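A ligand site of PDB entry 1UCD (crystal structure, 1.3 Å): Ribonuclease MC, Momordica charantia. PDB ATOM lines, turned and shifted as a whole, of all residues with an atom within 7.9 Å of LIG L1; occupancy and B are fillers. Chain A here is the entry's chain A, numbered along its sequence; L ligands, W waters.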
ATOM      1  N   PHE A   4       6.488 -21.183  15.299  1.00  0.00           N
ATOM      2  CA  PHE A   4       6.989 -19.897  14.844  1.00  0.00           C
ATOM      3  C   PHE A   4       5.937 -18.826  14.970  1.00  0.00           C
ATOM      4  O   PHE A   4       4.738 -19.083  14.826  1.00  0.00           O
ATOM      5  CB  PHE A   4       7.315 -19.889  13.351  1.00  0.00           C
ATOM      6  CG  PHE A   4       8.522 -20.653  12.941  1.00  0.00           C
ATOM      7  CD1 PHE A   4       8.385 -21.888  12.322  1.00  0.00           C
ATOM      8  CD2 PHE A   4       9.783 -20.096  13.072  1.00  0.00           C
ATOM      9  CE1 PHE A   4       9.493 -22.551  11.819  1.00  0.00           C
ATOM     10  CE2 PHE A   4      10.907 -20.765  12.571  1.00  0.00           C
ATOM     11  CZ  PHE A   4      10.756 -21.993  11.936  1.00  0.00           C
ATOM     12  N   TRP A   5       6.404 -17.625  15.221  1.00  0.00           N
ATOM     13  CA  TRP A   5       5.554 -16.450  15.231  1.00  0.00           C
ATOM     14  C   TRP A   5       6.068 -15.686  14.025  1.00  0.00           C
ATOM     15  O   TRP A   5       7.213 -15.219  14.029  1.00  0.00           O
ATOM     16  CB  TRP A   5       5.764 -15.609  16.479  1.00  0.00           C
ATOM     17  CG  TRP A   5       4.898 -15.991  17.614  1.00  0.00           C
ATOM     18  CD1 TRP A   5       4.396 -17.226  17.879  1.00  0.00           C
ATOM     19  CD2 TRP A   5       4.490 -15.138  18.685  1.00  0.00           C
ATOM     20  NE1 TRP A   5       3.693 -17.200  19.063  1.00  0.00           N
ATOM     21  CE2 TRP A   5       3.744 -15.932  19.578  1.00  0.00           C
ATOM     22  CE3 TRP A   5       4.693 -13.785  18.973  1.00  0.00           C
ATOM     23  CZ2 TRP A   5       3.185 -15.418  20.752  1.00  0.00           C
ATOM     24  CZ3 TRP A   5       4.137 -13.269  20.133  1.00  0.00           C
ATOM     25  CH2 TRP A   5       3.399 -14.081  21.011  1.00  0.00           C
ATOM     26  N   VAL A   7       5.903 -12.546  12.429  1.00  0.00           N
ATOM     27  CA  VAL A   7       5.465 -11.221  12.806  1.00  0.00           C
ATOM     28  C   VAL A   7       5.589 -10.178  11.730  1.00  0.00           C
ATOM     29  O   VAL A   7       6.676  -9.880  11.248  1.00  0.00           O
ATOM     30  CB  VAL A   7       6.259 -10.746  14.049  1.00  0.00           C
ATOM     31  CG1 VAL A   7       5.697  -9.442  14.563  1.00  0.00           C
ATOM     32  CG2 VAL A   7       6.232 -11.814  15.124  1.00  0.00           C
ATOM     33  N   LEU A  36      10.657 -13.560  12.009  1.00  0.00           N
ATOM     34  CA  LEU A  36      10.122 -14.902  12.129  1.00  0.00           C
ATOM     35  C   LEU A  36      10.743 -15.361  13.429  1.00  0.00           C
ATOM     36  O   LEU A  36      11.951 -15.599  13.528  1.00  0.00           O
ATOM     37  CB  LEU A  36      10.564 -15.750  10.948  1.00  0.00           C
ATOM     38  CG  LEU A  36      10.114 -17.209  10.978  1.00  0.00           C
ATOM     39  CD1 LEU A  36       8.607 -17.298  11.167  1.00  0.00           C
ATOM     40  CD2 LEU A  36      10.531 -17.882   9.680  1.00  0.00           C
ATOM     41  N   TRP A  37       9.913 -15.499  14.456  1.00  0.00           N
ATOM     42  CA  TRP A  37      10.406 -15.830  15.777  1.00  0.00           C
ATOM     43  C   TRP A  37      10.126 -17.231  16.256  1.00  0.00           C
ATOM     44  O   TRP A  37       8.982 -17.578  16.551  1.00  0.00           O
ATOM     45  CB  TRP A  37       9.832 -14.855  16.797  1.00  0.00           C
ATOM     46  CG  TRP A  37      10.034 -13.419  16.453  1.00  0.00           C
ATOM     47  CD1 TRP A  37      10.928 -12.896  15.558  1.00  0.00           C
ATOM     48  CD2 TRP A  37       9.335 -12.312  17.027  1.00  0.00           C
ATOM     49  NE1 TRP A  37      10.836 -11.518  15.557  1.00  0.00           N
ATOM     50  CE2 TRP A  37       9.860 -11.139  16.450  1.00  0.00           C
ATOM     51  CE3 TRP A  37       8.309 -12.200  17.981  1.00  0.00           C
ATOM     52  CZ2 TRP A  37       9.404  -9.858  16.785  1.00  0.00           C
ATOM     53  CZ3 TRP A  37       7.862 -10.928  18.323  1.00  0.00           C
ATOM     54  CH2 TRP A  37       8.405  -9.779  17.725  1.00  0.00           C
ATOM     55  N   PRO A  38      11.168 -18.066  16.359  1.00  0.00           N
ATOM     56  CA  PRO A  38      10.959 -19.427  16.831  1.00  0.00           C
ATOM     57  C   PRO A  38      10.443 -19.381  18.263  1.00  0.00           C
ATOM     58  O   PRO A  38      10.831 -18.520  19.046  1.00  0.00           O
ATOM     59  CB  PRO A  38      12.342 -20.043  16.743  1.00  0.00           C
ATOM     60  CG  PRO A  38      12.962 -19.303  15.603  1.00  0.00           C
ATOM     61  CD  PRO A  38      12.547 -17.884  15.877  1.00  0.00           C
ATOM     62  N   GLN A  39       9.576 -20.327  18.590  1.00  0.00           N
ATOM     63  CA  GLN A  39       8.983 -20.423  19.925  1.00  0.00           C
ATOM     64  C   GLN A  39       9.250 -21.810  20.478  1.00  0.00           C
ATOM     65  O   GLN A  39       9.509 -22.752  19.741  1.00  0.00           O
ATOM     66  CB  GLN A  39       7.469 -20.253  19.850  1.00  0.00           C
ATOM     67  CG  GLN A  39       6.987 -19.031  19.088  1.00  0.00           C
ATOM     68  CD  GLN A  39       7.242 -17.747  19.838  1.00  0.00           C
ATOM     69  OE1 GLN A  39       6.837 -17.584  20.983  1.00  0.00           O
ATOM     70  NE2 GLN A  39       7.928 -16.816  19.186  1.00  0.00           N
ATOM     71  N   GLN A  40       9.162 -21.919  21.799  1.00  0.00           N
ATOM     72  CA  GLN A  40       9.358 -23.187  22.481  1.00  0.00           C
ATOM     73  C   GLN A  40       8.495 -23.168  23.740  1.00  0.00           C
ATOM     74  O   GLN A  40       8.652 -22.302  24.594  1.00  0.00           O
ATOM     75  CB  GLN A  40      10.819 -23.377  22.877  1.00  0.00           C
ATOM     76  CG  GLN A  40      11.113 -24.729  23.517  1.00  0.00           C
ATOM     77  CD  GLN A  40      11.028 -25.870  22.520  1.00  0.00           C
ATOM     78  OE1 GLN A  40      11.802 -25.939  21.573  1.00  0.00           O
ATOM     79  NE2 GLN A  40      10.087 -26.780  22.745  1.00  0.00           N
ATOM     80  N   SER A  41       7.572 -24.108  23.836  1.00  0.00           N
ATOM     81  CA  SER A  41       6.692 -24.214  25.001  1.00  0.00           C
ATOM     82  C   SER A  41       6.043 -22.887  25.388  1.00  0.00           C
ATOM     83  O   SER A  41       6.089 -22.483  26.555  1.00  0.00           O
ATOM     84  CB  SER A  41       7.476 -24.779  26.181  1.00  0.00           C
ATOM     85  OG  SER A  41       8.018 -26.047  25.884  1.00  0.00           O
ATOM     86  N   GLY A  42       5.458 -22.203  24.409  1.00  0.00           N
ATOM     87  CA  GLY A  42       4.795 -20.937  24.680  1.00  0.00           C
ATOM     88  C   GLY A  42       5.674 -19.724  24.941  1.00  0.00           C
ATOM     89  O   GLY A  42       5.192 -18.721  25.468  1.00  0.00           O
ATOM     90  N   THR A  43       6.941 -19.808  24.574  1.00  0.00           N
ATOM     91  CA  THR A  43       7.844 -18.670  24.782  1.00  0.00           C
ATOM     92  C   THR A  43       8.792 -18.481  23.606  1.00  0.00           C
ATOM     93  O   THR A  43       9.143 -19.441  22.918  1.00  0.00           O
ATOM     94  CB  THR A  43       8.670 -18.843  26.084  1.00  0.00           C
ATOM     95  OG1 THR A  43       9.405 -17.640  26.335  1.00  0.00           O
ATOM     96  CG2 THR A  43       9.649 -19.996  25.946  1.00  0.00           C
ATOM     97  N   SER A  44       9.204 -17.242  23.378  1.00  0.00           N
ATOM     98  CA  SER A  44      10.109 -16.924  22.286  1.00  0.00           C
ATOM     99  C   SER A  44      11.529 -17.371  22.587  1.00  0.00           C
ATOM    100  O   SER A  44      12.063 -17.106  23.660  1.00  0.00           O
ATOM    101  CB  SER A  44      10.101 -15.426  22.015  1.00  0.00           C
ATOM    102  OG  SER A  44      10.925 -15.099  20.904  1.00  0.00           O
ATOM    103  N   LEU A  45      12.143 -18.035  21.616  1.00  0.00           N
ATOM    104  CA  LEU A  45      13.511 -18.499  21.748  1.00  0.00           C
ATOM    105  C   LEU A  45      14.386 -17.462  21.086  1.00  0.00           C
ATOM    106  O   LEU A  45      14.237 -17.197  19.893  1.00  0.00           O
ATOM    107  CB  LEU A  45      13.709 -19.845  21.050  1.00  0.00           C
ATOM    108  CG  LEU A  45      12.972 -21.028  21.664  1.00  0.00           C
ATOM    109  CD1 LEU A  45      13.207 -22.262  20.802  1.00  0.00           C
ATOM    110  CD2 LEU A  45      13.481 -21.266  23.082  1.00  0.00           C
ATOM    111  N   THR A  46      15.298 -16.868  21.841  1.00  0.00           N
ATOM    112  CA  THR A  46      16.163 -15.838  21.284  1.00  0.00           C
ATOM    113  C   THR A  46      17.641 -16.019  21.568  1.00  0.00           C
ATOM    114  O   THR A  46      18.038 -16.722  22.508  1.00  0.00           O
ATOM    115  CB  THR A  46      15.767 -14.447  21.818  1.00  0.00           C
ATOM    116  OG1 THR A  46      15.885 -14.431  23.248  1.00  0.00           O
ATOM    117  CG2 THR A  46      14.349 -14.109  21.421  1.00  0.00           C
ATOM    118  N   HIS A  88      16.735 -14.185  16.446  1.00  0.00           N
ATOM    119  CA  HIS A  88      15.673 -15.173  16.277  1.00  0.00           C
ATOM    120  C   HIS A  88      15.984 -16.352  15.369  1.00  0.00           C
ATOM    121  O   HIS A  88      15.766 -17.502  15.744  1.00  0.00           O
ATOM    122  CB  HIS A  88      14.423 -14.480  15.739  1.00  0.00           C
ATOM    123  CG  HIS A  88      13.942 -13.356  16.601  1.00  0.00           C
ATOM    124  ND1 HIS A  88      13.242 -13.547  17.766  1.00  0.00           N
ATOM    125  CD2 HIS A  88      14.051 -12.008  16.443  1.00  0.00           C
ATOM    126  CE1 HIS A  88      12.925 -12.383  18.291  1.00  0.00           C
ATOM    127  NE2 HIS A  88      13.406 -11.430  17.508  1.00  0.00           N
ATOM    128  N   ARG A 150      -0.702  -7.425  18.013  1.00  0.00           N
ATOM    129  CA  ARG A 150       0.181  -6.710  18.905  1.00  0.00           C
ATOM    130  C   ARG A 150       0.014  -5.221  18.743  1.00  0.00           C
ATOM    131  O   ARG A 150      -0.008  -4.685  17.632  1.00  0.00           O
ATOM    132  CB  ARG A 150       1.619  -7.136  18.642  1.00  0.00           C
ATOM    133  CG  ARG A 150       1.856  -8.604  18.996  1.00  0.00           C
ATOM    134  CD  ARG A 150       3.128  -9.142  18.387  1.00  0.00           C
ATOM    135  NE  ARG A 150       4.330  -8.519  18.939  1.00  0.00           N
ATOM    136  CZ  ARG A 150       4.822  -8.772  20.152  1.00  0.00           C
ATOM    137  NH1 ARG A 150       4.213  -9.627  20.960  1.00  0.00           N
ATOM    138  NH2 ARG A 150       5.933  -8.166  20.537  1.00  0.00           N
ATOM    139  N   VAL A 166       0.561 -11.232  13.977  1.00  0.00           N
ATOM    140  CA  VAL A 166       1.319 -12.456  14.013  1.00  0.00           C
ATOM    141  C   VAL A 166       0.540 -13.602  13.393  1.00  0.00           C
ATOM    142  O   VAL A 166      -0.654 -13.774  13.661  1.00  0.00           O
ATOM    143  CB  VAL A 166       1.651 -12.859  15.467  1.00  0.00           C
ATOM    144  CG1 VAL A 166       2.521 -14.092  15.477  1.00  0.00           C
ATOM    145  CG2 VAL A 166       2.321 -11.707  16.185  1.00  0.00           C
ATOM    146  N   THR A 180      -2.544 -17.382  20.084  1.00  0.00           N
ATOM    147  CA  THR A 180      -3.381 -17.185  21.263  1.00  0.00           C
ATOM    148  C   THR A 180      -2.937 -15.965  22.052  1.00  0.00           C
ATOM    149  O   THR A 180      -3.677 -15.465  22.901  1.00  0.00           O
ATOM    150  CB  THR A 180      -3.335 -18.403  22.200  1.00  0.00           C
ATOM    151  OG1 THR A 180      -1.964 -18.689  22.536  1.00  0.00           O
ATOM    152  CG2 THR A 180      -3.971 -19.611  21.540  1.00  0.00           C
ATOM    153  N   ARG A 181      -1.737 -15.479  21.772  1.00  0.00           N
ATOM    154  CA  ARG A 181      -1.184 -14.339  22.498  1.00  0.00           C
ATOM    155  C   ARG A 181      -1.251 -13.002  21.778  1.00  0.00           C
ATOM    156  O   ARG A 181      -0.649 -12.824  20.719  1.00  0.00           O
ATOM    157  CB  ARG A 181       0.268 -14.625  22.876  1.00  0.00           C
ATOM    158  CG  ARG A 181       0.471 -15.906  23.667  1.00  0.00           C
ATOM    159  CD  ARG A 181      -0.273 -15.857  24.998  1.00  0.00           C
ATOM    160  NE  ARG A 181       0.187 -14.749  25.829  1.00  0.00           N
ATOM    161  CZ  ARG A 181       1.396 -14.652  26.355  1.00  0.00           C
ATOM    162  NH1 ARG A 181       2.292 -15.617  26.149  1.00  0.00           N
ATOM    163  NH2 ARG A 181       1.717 -13.610  27.107  1.00  0.00           N
ATOM    164  N   THR A 183      -1.101  -8.593  22.443  1.00  0.00           N
ATOM    165  CA  THR A 183      -0.674  -7.584  23.397  1.00  0.00           C
ATOM    166  C   THR A 183      -1.707  -6.464  23.271  1.00  0.00           C
ATOM    167  O   THR A 183      -1.716  -5.528  24.069  1.00  0.00           O
ATOM    168  CB  THR A 183       0.737  -7.028  23.120  1.00  0.00           C
ATOM    169  OG1 THR A 183       0.821  -6.534  21.785  1.00  0.00           O
ATOM    170  CG2 THR A 183       1.782  -8.117  23.344  1.00  0.00           C
HETATM  171  N1  LIG L   1       5.735 -13.683  23.809  1.00  0.00           N
HETATM  172  C1  LIG L   1       5.835 -14.938  23.226  1.00  0.00           C
HETATM  173  O1  LIG L   1       5.289 -15.886  23.748  1.00  0.00           O
HETATM  174  N2  LIG L   1       6.578 -14.984  22.054  1.00  0.00           N
HETATM  175  C2  LIG L   1       7.219 -13.900  21.423  1.00  0.00           C
HETATM  176  O2  LIG L   1       7.839 -14.112  20.395  1.00  0.00           O
HETATM  177  C3  LIG L   1       7.061 -12.635  22.105  1.00  0.00           C
HETATM  178  C4  LIG L   1       6.350 -12.567  23.228  1.00  0.00           C
HETATM  179  N1  LG2 L   2      13.522  -2.695  14.328  1.00  0.00           N
HETATM  180  C1  LG2 L   2      14.220  -2.206  13.220  1.00  0.00           C
HETATM  181  N2  LG2 L   2      13.463  -2.021  12.088  1.00  0.00           N
HETATM  182  C2  LG2 L   2      12.091  -2.276  11.952  1.00  0.00           C
HETATM  183  C3  LG2 L   2      11.449  -2.773  13.134  1.00  0.00           C
HETATM  184  C4  LG2 L   2      12.154  -2.972  14.242  1.00  0.00           C
HETATM  185  O1  LG2 L   2      15.416  -1.966  13.282  1.00  0.00           O
HETATM  186  O2  LG2 L   2      11.582  -2.055  10.878  1.00  0.00           O
HETATM  187  C5  LG2 L   2      14.308  -2.918  15.555  1.00  0.00           C
HETATM  188  C6  LG2 L   2      13.906  -2.156  16.806  1.00  0.00           C
HETATM  189  O3  LG2 L   2      14.376  -0.797  16.813  1.00  0.00           O
HETATM  190  C7  LG2 L   2      14.420  -3.023  17.958  1.00  0.00           C
HETATM  191  C8  LG2 L   2      14.221  -4.414  17.379  1.00  0.00           C
HETATM  192  O4  LG2 L   2      15.799  -2.694  18.309  1.00  0.00           O
HETATM  193  O5  LG2 L   2      14.412  -4.269  15.935  1.00  0.00           O
HETATM  194  C9  LG2 L   2      12.869  -5.094  17.560  1.00  0.00           C
HETATM  195  O6  LG2 L   2      12.863  -6.445  17.088  1.00  0.00           O
HETATM  196  P1  LG2 L   2      13.173  -7.695  18.056  1.00  0.00           P
HETATM  197  O7  LG2 L   2      12.266  -7.883  19.253  1.00  0.00           O
HETATM  198  O8  LG2 L   2      14.549  -7.585  18.624  1.00  0.00           O
HETATM  199  O9  LG2 L   2      13.176  -8.931  16.964  1.00  0.00           O
HETATM  200  O   HOH W   1       8.607 -14.845  24.965  1.00  0.00           O
HETATM  201  O   HOH W   2       4.598 -18.332  22.353  1.00  0.00           O
HETATM  202  O   HOH W   3       4.067 -12.091  25.489  1.00  0.00           O
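Water W3 lies within hydrogen-bond range of N1 of LIG L1 and NH2 of Arg 181.
Water W1 lies within hydrogen-bond range of N of Ser 44 (2.9 Å), OG1 of Thr 43 (3.2 Å) and N1 of LIG L1 (3.3 Å).
The side-chain amide oxygen of Gln 39 is in hydrogen-bond range of the backbone NH of Ser 44 (3.4 Å).
The side-chain amide nitrogen (NE2) of Gln 39 sits at hydrogen-bond distance from the backbone carbonyl oxygen (O) of Trp 37, at 2.9 Å.
N of Trp 37 sits at hydrogen-bond distance from O of Trp 5 (2.7 Å).
The indole nitrogen (NE1) of Trp 37 is in hydrogen-bond range of a ring nitrogen (NE2) of His 88, 3.2 Å away.
A nitrogen (N2) of LIG L1 sits at hydrogen-bond distance from the side-chain amide oxygen of Gln 39 (2.8 Å).
The side-chain hydroxyl (OG) of Ser 44 lies close to an oxygen (O2) of LIG L1, 3.3 Å away.
An oxygen (O9) of LG2 L2 is in hydrogen-bond range of a ring nitrogen (NE2) of His 88.
O1 of LIG L1 sits close to O of Gly 42 (3.3 Å).
Residues that only touch LIG L1: Trp 5, Trp 37, Thr 43 and Arg 181.
Seven residues have an atom within 4 Å of LIG L1: Trp 5, Trp 37, Gln 39, Gly 42, Thr 43, Ser 44 and Arg 181.
The nearest printed residue that does not touch LIG L1 is Arg 150 (4.3 Å).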
